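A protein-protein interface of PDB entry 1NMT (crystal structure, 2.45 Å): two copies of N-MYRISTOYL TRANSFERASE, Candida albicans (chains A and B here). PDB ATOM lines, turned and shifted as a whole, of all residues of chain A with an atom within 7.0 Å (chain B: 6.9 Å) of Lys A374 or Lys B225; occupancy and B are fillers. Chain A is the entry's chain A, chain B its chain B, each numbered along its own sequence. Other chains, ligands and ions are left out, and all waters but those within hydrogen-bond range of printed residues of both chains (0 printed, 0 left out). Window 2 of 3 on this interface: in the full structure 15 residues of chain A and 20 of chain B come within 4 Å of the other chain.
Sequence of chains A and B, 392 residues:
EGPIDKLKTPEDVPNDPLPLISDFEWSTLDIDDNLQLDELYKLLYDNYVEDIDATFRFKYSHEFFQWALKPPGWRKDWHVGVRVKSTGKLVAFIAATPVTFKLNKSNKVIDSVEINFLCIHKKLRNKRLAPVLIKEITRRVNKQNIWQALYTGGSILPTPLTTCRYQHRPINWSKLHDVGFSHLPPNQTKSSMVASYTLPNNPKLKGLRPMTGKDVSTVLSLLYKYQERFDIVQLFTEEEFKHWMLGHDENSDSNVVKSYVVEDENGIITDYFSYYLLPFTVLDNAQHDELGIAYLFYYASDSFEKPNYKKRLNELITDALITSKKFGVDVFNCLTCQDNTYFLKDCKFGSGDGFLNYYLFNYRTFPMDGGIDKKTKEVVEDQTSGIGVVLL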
ATOM      1  N   PRO A 158     -16.907   8.979 -14.176  1.00  0.00           N
ATOM      2  CA  PRO A 158     -16.686   7.601 -14.629  1.00  0.00           C
ATOM      3  C   PRO A 158     -15.777   7.594 -15.872  1.00  0.00           C
ATOM      4  O   PRO A 158     -15.731   8.573 -16.620  1.00  0.00           O
ATOM      5  CB  PRO A 158     -18.093   7.088 -14.970  1.00  0.00           C
ATOM      6  CG  PRO A 158     -19.048   8.131 -14.426  1.00  0.00           C
ATOM      7  CD  PRO A 158     -18.295   9.423 -14.357  1.00  0.00           C
ATOM      8  N   THR A 159     -15.021   6.512 -16.042  1.00  0.00           N
ATOM      9  CA  THR A 159     -14.168   6.307 -17.215  1.00  0.00           C
ATOM     10  C   THR A 159     -13.152   7.354 -17.753  1.00  0.00           C
ATOM     11  O   THR A 159     -13.270   7.833 -18.879  1.00  0.00           O
ATOM     12  CB  THR A 159     -15.073   5.886 -18.388  1.00  0.00           C
ATOM     13  OG1 THR A 159     -15.863   7.007 -18.797  1.00  0.00           O
ATOM     14  CG2 THR A 159     -16.016   4.784 -17.957  1.00  0.00           C
ATOM     15  N   PRO A 160     -12.177   7.762 -16.937  1.00  0.00           N
ATOM     16  CA  PRO A 160     -11.152   8.725 -17.378  1.00  0.00           C
ATOM     17  C   PRO A 160     -10.182   7.969 -18.313  1.00  0.00           C
ATOM     18  O   PRO A 160     -10.158   6.744 -18.272  1.00  0.00           O
ATOM     19  CB  PRO A 160     -10.446   9.116 -16.079  1.00  0.00           C
ATOM     20  CG  PRO A 160     -10.675   7.941 -15.167  1.00  0.00           C
ATOM     21  CD  PRO A 160     -12.026   7.389 -15.520  1.00  0.00           C
ATOM     22  N   THR A 162      -7.137   7.927 -17.976  1.00  0.00           N
ATOM     23  CA  THR A 162      -6.267   7.365 -16.965  1.00  0.00           C
ATOM     24  C   THR A 162      -6.080   8.415 -15.867  1.00  0.00           C
ATOM     25  O   THR A 162      -6.761   9.437 -15.855  1.00  0.00           O
ATOM     26  CB  THR A 162      -4.880   6.965 -17.561  1.00  0.00           C
ATOM     27  OG1 THR A 162      -4.066   6.407 -16.527  1.00  0.00           O
ATOM     28  CG2 THR A 162      -4.143   8.177 -18.125  1.00  0.00           C
ATOM     29  N   THR A 163      -5.162   8.163 -14.948  1.00  0.00           N
ATOM     30  CA  THR A 163      -4.908   9.094 -13.872  1.00  0.00           C
ATOM     31  C   THR A 163      -3.401   9.160 -13.647  1.00  0.00           C
ATOM     32  O   THR A 163      -2.729   8.138 -13.616  1.00  0.00           O
ATOM     33  CB  THR A 163      -5.585   8.606 -12.575  1.00  0.00           C
ATOM     34  OG1 THR A 163      -6.981   8.369 -12.820  1.00  0.00           O
ATOM     35  CG2 THR A 163      -5.398   9.632 -11.445  1.00  0.00           C
ATOM     36  N   PRO A 367      -7.711   1.485 -22.333  1.00  0.00           N
ATOM     37  CA  PRO A 367      -7.103   1.946 -21.068  1.00  0.00           C
ATOM     38  C   PRO A 367      -5.676   2.439 -21.329  1.00  0.00           C
ATOM     39  O   PRO A 367      -5.038   2.000 -22.287  1.00  0.00           O
ATOM     40  CB  PRO A 367      -7.116   0.703 -20.168  1.00  0.00           C
ATOM     41  CG  PRO A 367      -8.156  -0.221 -20.799  1.00  0.00           C
ATOM     42  CD  PRO A 367      -8.127   0.072 -22.287  1.00  0.00           C
ATOM     43  N   MET A 368      -5.179   3.348 -20.493  1.00  0.00           N
ATOM     44  CA  MET A 368      -3.830   3.884 -20.667  1.00  0.00           C
ATOM     45  C   MET A 368      -3.097   3.841 -19.343  1.00  0.00           C
ATOM     46  O   MET A 368      -3.730   3.985 -18.298  1.00  0.00           O
ATOM     47  CB  MET A 368      -3.898   5.331 -21.127  1.00  0.00           C
ATOM     48  CG  MET A 368      -4.432   5.515 -22.498  1.00  0.00           C
ATOM     49  SD  MET A 368      -4.296   7.222 -22.953  1.00  0.00           S
ATOM     50  CE  MET A 368      -5.161   7.153 -24.516  1.00  0.00           C
ATOM     51  N   ILE A 372       1.547   5.135 -12.658  1.00  0.00           N
ATOM     52  CA  ILE A 372       1.393   4.726 -11.262  1.00  0.00           C
ATOM     53  C   ILE A 372       0.698   3.377 -11.244  1.00  0.00           C
ATOM     54  O   ILE A 372       0.048   3.003 -12.211  1.00  0.00           O
ATOM     55  CB  ILE A 372       0.542   5.751 -10.420  1.00  0.00           C
ATOM     56  CG1 ILE A 372      -0.852   5.927 -11.035  1.00  0.00           C
ATOM     57  CG2 ILE A 372       1.276   7.097 -10.316  1.00  0.00           C
ATOM     58  CD1 ILE A 372      -1.709   6.962 -10.262  1.00  0.00           C
ATOM     59  N   ASP A 373       0.857   2.642 -10.149  1.00  0.00           N
ATOM     60  CA  ASP A 373       0.207   1.350 -10.022  1.00  0.00           C
ATOM     61  C   ASP A 373      -1.301   1.563  -9.910  1.00  0.00           C
ATOM     62  O   ASP A 373      -1.794   2.315  -9.035  1.00  0.00           O
ATOM     63  CB  ASP A 373       0.713   0.613  -8.781  1.00  0.00           C
ATOM     64  CG  ASP A 373      -0.071  -0.641  -8.504  1.00  0.00           C
ATOM     65  OD1 ASP A 373       0.045  -1.569  -9.323  1.00  0.00           O
ATOM     66  OD2 ASP A 373      -0.797  -0.692  -7.482  1.00  0.00           O
ATOM     67  N   LYS A 374      -2.008   0.876 -10.802  1.00  0.00           N
ATOM     68  CA  LYS A 374      -3.450   0.936 -10.878  1.00  0.00           C
ATOM     69  C   LYS A 374      -4.157   0.610  -9.553  1.00  0.00           C
ATOM     70  O   LYS A 374      -5.367   0.794  -9.429  1.00  0.00           O
ATOM     71  CB  LYS A 374      -3.924  -0.004 -11.974  1.00  0.00           C
ATOM     72  CG  LYS A 374      -5.431   0.006 -12.193  1.00  0.00           C
ATOM     73  CD  LYS A 374      -5.931   1.301 -12.859  1.00  0.00           C
ATOM     74  CE  LYS A 374      -7.466   1.438 -12.744  1.00  0.00           C
ATOM     75  NZ  LYS A 374      -8.224   1.240 -14.033  1.00  0.00           N
ATOM     76  N   LYS A 375      -3.416   0.147  -8.553  1.00  0.00           N
ATOM     77  CA  LYS A 375      -4.033  -0.182  -7.278  1.00  0.00           C
ATOM     78  C   LYS A 375      -3.515   0.592  -6.086  1.00  0.00           C
ATOM     79  O   LYS A 375      -4.310   1.011  -5.256  1.00  0.00           O
ATOM     80  CB  LYS A 375      -3.862  -1.651  -6.979  1.00  0.00           C
ATOM     81  CG  LYS A 375      -4.468  -2.564  -7.987  1.00  0.00           C
ATOM     82  CD  LYS A 375      -4.434  -3.956  -7.406  1.00  0.00           C
ATOM     83  CE  LYS A 375      -4.683  -5.013  -8.447  1.00  0.00           C
ATOM     84  NZ  LYS A 375      -4.685  -6.350  -7.783  1.00  0.00           N
ATOM     85  N   THR A 376      -2.195   0.761  -5.987  1.00  0.00           N
ATOM     86  CA  THR A 376      -1.553   1.483  -4.887  1.00  0.00           C
ATOM     87  C   THR A 376      -1.418   2.984  -5.162  1.00  0.00           C
ATOM     88  O   THR A 376      -1.177   3.770  -4.230  1.00  0.00           O
ATOM     89  CB  THR A 376      -0.130   0.947  -4.643  1.00  0.00           C
ATOM     90  OG1 THR A 376       0.699   1.302  -5.758  1.00  0.00           O
ATOM     91  CG2 THR A 376      -0.135  -0.568  -4.494  1.00  0.00           C
ATOM     92  N   LYS A 377      -1.555   3.362  -6.441  1.00  0.00           N
ATOM     93  CA  LYS A 377      -1.427   4.761  -6.909  1.00  0.00           C
ATOM     94  C   LYS A 377      -0.005   5.256  -6.709  1.00  0.00           C
ATOM     95  O   LYS A 377       0.251   6.466  -6.731  1.00  0.00           O
ATOM     96  CB  LYS A 377      -2.380   5.722  -6.162  1.00  0.00           C
ATOM     97  CG  LYS A 377      -3.759   5.190  -5.921  1.00  0.00           C
ATOM     98  CD  LYS A 377      -4.364   4.635  -7.209  1.00  0.00           C
ATOM     99  CE  LYS A 377      -5.721   5.260  -7.466  1.00  0.00           C
ATOM    100  NZ  LYS A 377      -6.691   4.203  -7.775  1.00  0.00           N
ATOM    101  N   GLU A 378       0.915   4.322  -6.482  1.00  0.00           N
ATOM    102  CA  GLU A 378       2.309   4.680  -6.277  1.00  0.00           C
ATOM    103  C   GLU A 378       3.052   4.693  -7.615  1.00  0.00           C
ATOM    104  O   GLU A 378       2.691   3.984  -8.582  1.00  0.00           O
ATOM    105  CB  GLU A 378       2.990   3.699  -5.313  1.00  0.00           C
ATOM    106  CG  GLU A 378       2.376   3.624  -3.931  1.00  0.00           C
ATOM    107  CD  GLU A 378       2.431   4.950  -3.192  1.00  0.00           C
ATOM    108  OE1 GLU A 378       3.535   5.526  -3.072  1.00  0.00           O
ATOM    109  OE2 GLU A 378       1.359   5.418  -2.734  1.00  0.00           O
ATOM    110  N   VAL A 380       5.316   3.955 -10.601  1.00  0.00           N
ATOM    111  CA  VAL A 380       5.887   2.737 -11.169  1.00  0.00           C
ATOM    112  C   VAL A 380       7.098   3.174 -12.038  1.00  0.00           C
ATOM    113  O   VAL A 380       6.937   3.682 -13.143  1.00  0.00           O
ATOM    114  CB  VAL A 380       4.877   1.992 -12.048  1.00  0.00           C
ATOM    115  CG1 VAL A 380       5.601   0.972 -12.898  1.00  0.00           C
ATOM    116  CG2 VAL A 380       3.851   1.280 -11.172  1.00  0.00           C
ATOM    117  N   VAL B 219     -13.404   4.412  -2.899  1.00  0.00           N
ATOM    118  CA  VAL B 219     -14.679   3.703  -2.921  1.00  0.00           C
ATOM    119  C   VAL B 219     -15.499   4.230  -4.100  1.00  0.00           C
ATOM    120  O   VAL B 219     -16.086   3.462  -4.878  1.00  0.00           O
ATOM    121  CB  VAL B 219     -15.461   3.902  -1.590  1.00  0.00           C
ATOM    122  CG1 VAL B 219     -16.841   3.265  -1.690  1.00  0.00           C
ATOM    123  CG2 VAL B 219     -14.690   3.297  -0.450  1.00  0.00           C
ATOM    124  N   LEU B 220     -15.507   5.545  -4.249  1.00  0.00           N
ATOM    125  CA  LEU B 220     -16.257   6.157  -5.332  1.00  0.00           C
ATOM    126  C   LEU B 220     -15.854   5.550  -6.680  1.00  0.00           C
ATOM    127  O   LEU B 220     -16.715   5.201  -7.506  1.00  0.00           O
ATOM    128  CB  LEU B 220     -16.029   7.675  -5.336  1.00  0.00           C
ATOM    129  CG  LEU B 220     -17.022   8.450  -6.206  1.00  0.00           C
ATOM    130  CD1 LEU B 220     -18.476   8.088  -5.838  1.00  0.00           C
ATOM    131  CD2 LEU B 220     -16.772   9.920  -6.017  1.00  0.00           C
ATOM    132  N   SER B 221     -14.549   5.417  -6.909  1.00  0.00           N
ATOM    133  CA  SER B 221     -14.070   4.836  -8.171  1.00  0.00           C
ATOM    134  C   SER B 221     -14.501   3.383  -8.275  1.00  0.00           C
ATOM    135  O   SER B 221     -14.862   2.902  -9.353  1.00  0.00           O
ATOM    136  CB  SER B 221     -12.542   4.890  -8.281  1.00  0.00           C
ATOM    137  OG  SER B 221     -12.062   6.224  -8.284  1.00  0.00           O
ATOM    138  N   LEU B 222     -14.433   2.668  -7.157  1.00  0.00           N
ATOM    139  CA  LEU B 222     -14.853   1.281  -7.156  1.00  0.00           C
ATOM    140  C   LEU B 222     -16.354   1.206  -7.535  1.00  0.00           C
ATOM    141  O   LEU B 222     -16.727   0.436  -8.414  1.00  0.00           O
ATOM    142  CB  LEU B 222     -14.600   0.673  -5.776  1.00  0.00           C
ATOM    143  CG  LEU B 222     -15.089  -0.770  -5.640  1.00  0.00           C
ATOM    144  CD1 LEU B 222     -14.170  -1.716  -6.416  1.00  0.00           C
ATOM    145  CD2 LEU B 222     -15.121  -1.146  -4.168  1.00  0.00           C
ATOM    146  N   LEU B 223     -17.205   2.025  -6.897  1.00  0.00           N
ATOM    147  CA  LEU B 223     -18.639   2.029  -7.206  1.00  0.00           C
ATOM    148  C   LEU B 223     -18.875   2.413  -8.666  1.00  0.00           C
ATOM    149  O   LEU B 223     -19.704   1.791  -9.348  1.00  0.00           O
ATOM    150  CB  LEU B 223     -19.400   3.004  -6.285  1.00  0.00           C
ATOM    151  CG  LEU B 223     -20.895   3.267  -6.570  1.00  0.00           C
ATOM    152  CD1 LEU B 223     -21.693   1.990  -6.376  1.00  0.00           C
ATOM    153  CD2 LEU B 223     -21.424   4.376  -5.623  1.00  0.00           C
ATOM    154  N   TYR B 224     -18.137   3.411  -9.163  1.00  0.00           N
ATOM    155  CA  TYR B 224     -18.314   3.853 -10.562  1.00  0.00           C
ATOM    156  C   TYR B 224     -18.021   2.742 -11.578  1.00  0.00           C
ATOM    157  O   TYR B 224     -18.788   2.518 -12.523  1.00  0.00           O
ATOM    158  CB  TYR B 224     -17.438   5.062 -10.861  1.00  0.00           C
ATOM    159  CG  TYR B 224     -18.032   6.393 -10.424  1.00  0.00           C
ATOM    160  CD1 TYR B 224     -19.253   6.464  -9.710  1.00  0.00           C
ATOM    161  CD2 TYR B 224     -17.367   7.588 -10.704  1.00  0.00           C
ATOM    162  CE1 TYR B 224     -19.784   7.706  -9.291  1.00  0.00           C
ATOM    163  CE2 TYR B 224     -17.886   8.814 -10.295  1.00  0.00           C
ATOM    164  CZ  TYR B 224     -19.091   8.870  -9.591  1.00  0.00           C
ATOM    165  OH  TYR B 224     -19.563  10.105  -9.190  1.00  0.00           O
ATOM    166  N   LYS B 225     -16.915   2.028 -11.389  1.00  0.00           N
ATOM    167  CA  LYS B 225     -16.584   0.921 -12.297  1.00  0.00           C
ATOM    168  C   LYS B 225     -17.678  -0.138 -12.172  1.00  0.00           C
ATOM    169  O   LYS B 225     -18.204  -0.644 -13.165  1.00  0.00           O
ATOM    170  CB  LYS B 225     -15.253   0.269 -11.912  1.00  0.00           C
ATOM    171  CG  LYS B 225     -14.038   0.811 -12.637  1.00  0.00           C
ATOM    172  CD  LYS B 225     -12.755   0.531 -11.856  1.00  0.00           C
ATOM    173  CE  LYS B 225     -11.973   1.813 -11.561  1.00  0.00           C
ATOM    174  NZ  LYS B 225     -10.510   1.546 -11.548  1.00  0.00           N
ATOM    175  N   TYR B 226     -18.008  -0.476 -10.932  1.00  0.00           N
ATOM    176  CA  TYR B 226     -19.012  -1.486 -10.687  1.00  0.00           C
ATOM    177  C   TYR B 226     -20.406  -1.183 -11.241  1.00  0.00           C
ATOM    178  O   TYR B 226     -21.013  -2.022 -11.914  1.00  0.00           O
ATOM    179  CB  TYR B 226     -19.121  -1.747  -9.174  1.00  0.00           C
ATOM    180  CG  TYR B 226     -20.186  -2.759  -8.825  1.00  0.00           C
ATOM    181  CD1 TYR B 226     -19.993  -4.119  -9.081  1.00  0.00           C
ATOM    182  CD2 TYR B 226     -21.413  -2.354  -8.288  1.00  0.00           C
ATOM    183  CE1 TYR B 226     -21.007  -5.059  -8.814  1.00  0.00           C
ATOM    184  CE2 TYR B 226     -22.432  -3.279  -8.018  1.00  0.00           C
ATOM    185  CZ  TYR B 226     -22.227  -4.632  -8.284  1.00  0.00           C
ATOM    186  OH  TYR B 226     -23.230  -5.551  -8.013  1.00  0.00           O
ATOM    187  N   GLN B 227     -20.929   0.007 -10.968  1.00  0.00           N
ATOM    188  CA  GLN B 227     -22.303   0.295 -11.396  1.00  0.00           C
ATOM    189  C   GLN B 227     -22.561   0.484 -12.882  1.00  0.00           C
ATOM    190  O   GLN B 227     -23.687   0.795 -13.272  1.00  0.00           O
ATOM    191  CB  GLN B 227     -22.868   1.477 -10.614  1.00  0.00           C
ATOM    192  CG  GLN B 227     -22.292   2.829 -10.971  1.00  0.00           C
ATOM    193  CD  GLN B 227     -22.746   3.911  -9.999  1.00  0.00           C
ATOM    194  OE1 GLN B 227     -22.500   5.110 -10.204  1.00  0.00           O
ATOM    195  NE2 GLN B 227     -23.410   3.489  -8.927  1.00  0.00           N
ATOM    196  N   GLU B 228     -21.530   0.270 -13.704  1.00  0.00           N
ATOM    197  CA  GLU B 228     -21.669   0.402 -15.159  1.00  0.00           C
ATOM    198  C   GLU B 228     -22.717  -0.587 -15.683  1.00  0.00           C
ATOM    199  O   GLU B 228     -23.322  -0.369 -16.742  1.00  0.00           O
ATOM    200  CB  GLU B 228     -20.333   0.128 -15.890  1.00  0.00           C
ATOM    201  CG  GLU B 228     -19.302   1.199 -15.733  1.00  0.00           C
ATOM    202  CD  GLU B 228     -19.587   2.412 -16.587  1.00  0.00           C
ATOM    203  OE1 GLU B 228     -20.592   2.404 -17.336  1.00  0.00           O
ATOM    204  OE2 GLU B 228     -18.800   3.381 -16.508  1.00  0.00           O
ATOM    205  N   ARG B 229     -22.927  -1.665 -14.935  1.00  0.00           N
ATOM    206  CA  ARG B 229     -23.887  -2.721 -15.294  1.00  0.00           C
ATOM    207  C   ARG B 229     -25.380  -2.369 -15.145  1.00  0.00           C
ATOM    208  O   ARG B 229     -26.242  -3.074 -15.692  1.00  0.00           O
ATOM    209  CB  ARG B 229     -23.615  -3.956 -14.436  1.00  0.00           C
ATOM    210  CG  ARG B 229     -24.023  -3.725 -12.988  1.00  0.00           C
ATOM    211  CD  ARG B 229     -23.180  -4.519 -12.034  1.00  0.00           C
ATOM    212  NE  ARG B 229     -23.401  -5.944 -12.240  1.00  0.00           N
ATOM    213  CZ  ARG B 229     -22.509  -6.760 -12.788  1.00  0.00           C
ATOM    214  NH1 ARG B 229     -21.331  -6.282 -13.188  1.00  0.00           N
ATOM    215  NH2 ARG B 229     -22.804  -8.045 -12.940  1.00  0.00           N
ATOM    216  N   ILE B 268      -5.446  -2.843  -0.479  1.00  0.00           N
ATOM    217  CA  ILE B 268      -6.284  -2.316  -1.548  1.00  0.00           C
ATOM    218  C   ILE B 268      -7.764  -2.634  -1.325  1.00  0.00           C
ATOM    219  O   ILE B 268      -8.110  -3.778  -1.057  1.00  0.00           O
ATOM    220  CB  ILE B 268      -5.805  -2.911  -2.884  1.00  0.00           C
ATOM    221  CG1 ILE B 268      -4.412  -2.351  -3.186  1.00  0.00           C
ATOM    222  CG2 ILE B 268      -6.808  -2.618  -4.011  1.00  0.00           C
ATOM    223  CD1 ILE B 268      -3.653  -3.170  -4.196  1.00  0.00           C
ATOM    224  N   ALA B 300     -20.452  -2.385  -3.825  1.00  0.00           N
ATOM    225  CA  ALA B 300     -19.697  -2.680  -5.034  1.00  0.00           C
ATOM    226  C   ALA B 300     -18.606  -3.700  -4.753  1.00  0.00           C
ATOM    227  O   ALA B 300     -18.077  -3.773  -3.640  1.00  0.00           O
ATOM    228  CB  ALA B 300     -19.096  -1.400  -5.595  1.00  0.00           C
ATOM    229  N   SER B 301     -18.268  -4.487  -5.772  1.00  0.00           N
ATOM    230  CA  SER B 301     -17.240  -5.502  -5.633  1.00  0.00           C
ATOM    231  C   SER B 301     -16.312  -5.628  -6.849  1.00  0.00           C
ATOM    232  O   SER B 301     -16.728  -5.376  -7.973  1.00  0.00           O
ATOM    233  CB  SER B 301     -17.902  -6.837  -5.367  1.00  0.00           C
ATOM    234  OG  SER B 301     -16.942  -7.858  -5.409  1.00  0.00           O
ATOM    235  N   PHE B 304     -16.795  -8.626  -9.880  1.00  0.00           N
ATOM    236  CA  PHE B 304     -17.880  -8.742 -10.867  1.00  0.00           C
ATOM    237  C   PHE B 304     -17.504  -9.375 -12.191  1.00  0.00           C
ATOM    238  O   PHE B 304     -18.359  -9.935 -12.882  1.00  0.00           O
ATOM    239  CB  PHE B 304     -18.558  -7.402 -11.114  1.00  0.00           C
ATOM    240  CG  PHE B 304     -17.730  -6.430 -11.869  1.00  0.00           C
ATOM    241  CD1 PHE B 304     -17.786  -6.386 -13.256  1.00  0.00           C
ATOM    242  CD2 PHE B 304     -16.957  -5.484 -11.193  1.00  0.00           C
ATOM    243  CE1 PHE B 304     -17.093  -5.407 -13.968  1.00  0.00           C
ATOM    244  CE2 PHE B 304     -16.264  -4.505 -11.886  1.00  0.00           C
ATOM    245  CZ  PHE B 304     -16.334  -4.461 -13.286  1.00  0.00           C
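The side-chain amino group (NZ) of Lys A374 lies close to the side-chain amino group (NZ) of Lys B225 (3.4 Å).
Among the printed residues, merely in contact across the chains: Lys A375 with Ile B268, Thr A159 with Glu B228 and Pro A158 with Tyr B224.
Printed residues of chain B that touch a printed residue of chain A: Tyr B224, Lys B225, Glu B228 and Ile B268.
Of the 15 printed residues of chain A, 4 touch a printed residue of chain B.
Printed residues of chain A that touch a printed residue of chain B: Pro A158, Thr A159, Lys A374 and Lys A375.
Among the printed residues, 4 pairs touch across the chains.
Among the printed residues, no Asp or Glu carboxylate lies within 4 Å of a Lys or Arg side-chain nitrogen of the other chain.
No position is printed for both chains.
Of the 4 pairs that touch across the chains among the printed residues, none has its exchanged pair printed and touching as well.
OD2 of Asp A373 sits close to N of Lys A375, 3.0 Å away.
Lys A374 touches just one residue of chain B: Lys B225.
Lys B225 touches just one residue of chain A: Lys A374 (3.3 Å).
Of the printed residues of chain A, Ile B268 touches Lys A375 (3.2 Å).
Of the printed residues of chain A, Tyr B224 touches Pro A158.
Printed residues of chain B within 4 Å of Pro A158: Tyr B224.
Lys A377 touches none of the printed residues of chain B.
The nearest residue of chain B that does not touch Lys A374 is Ile B268 (6.6 Å).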
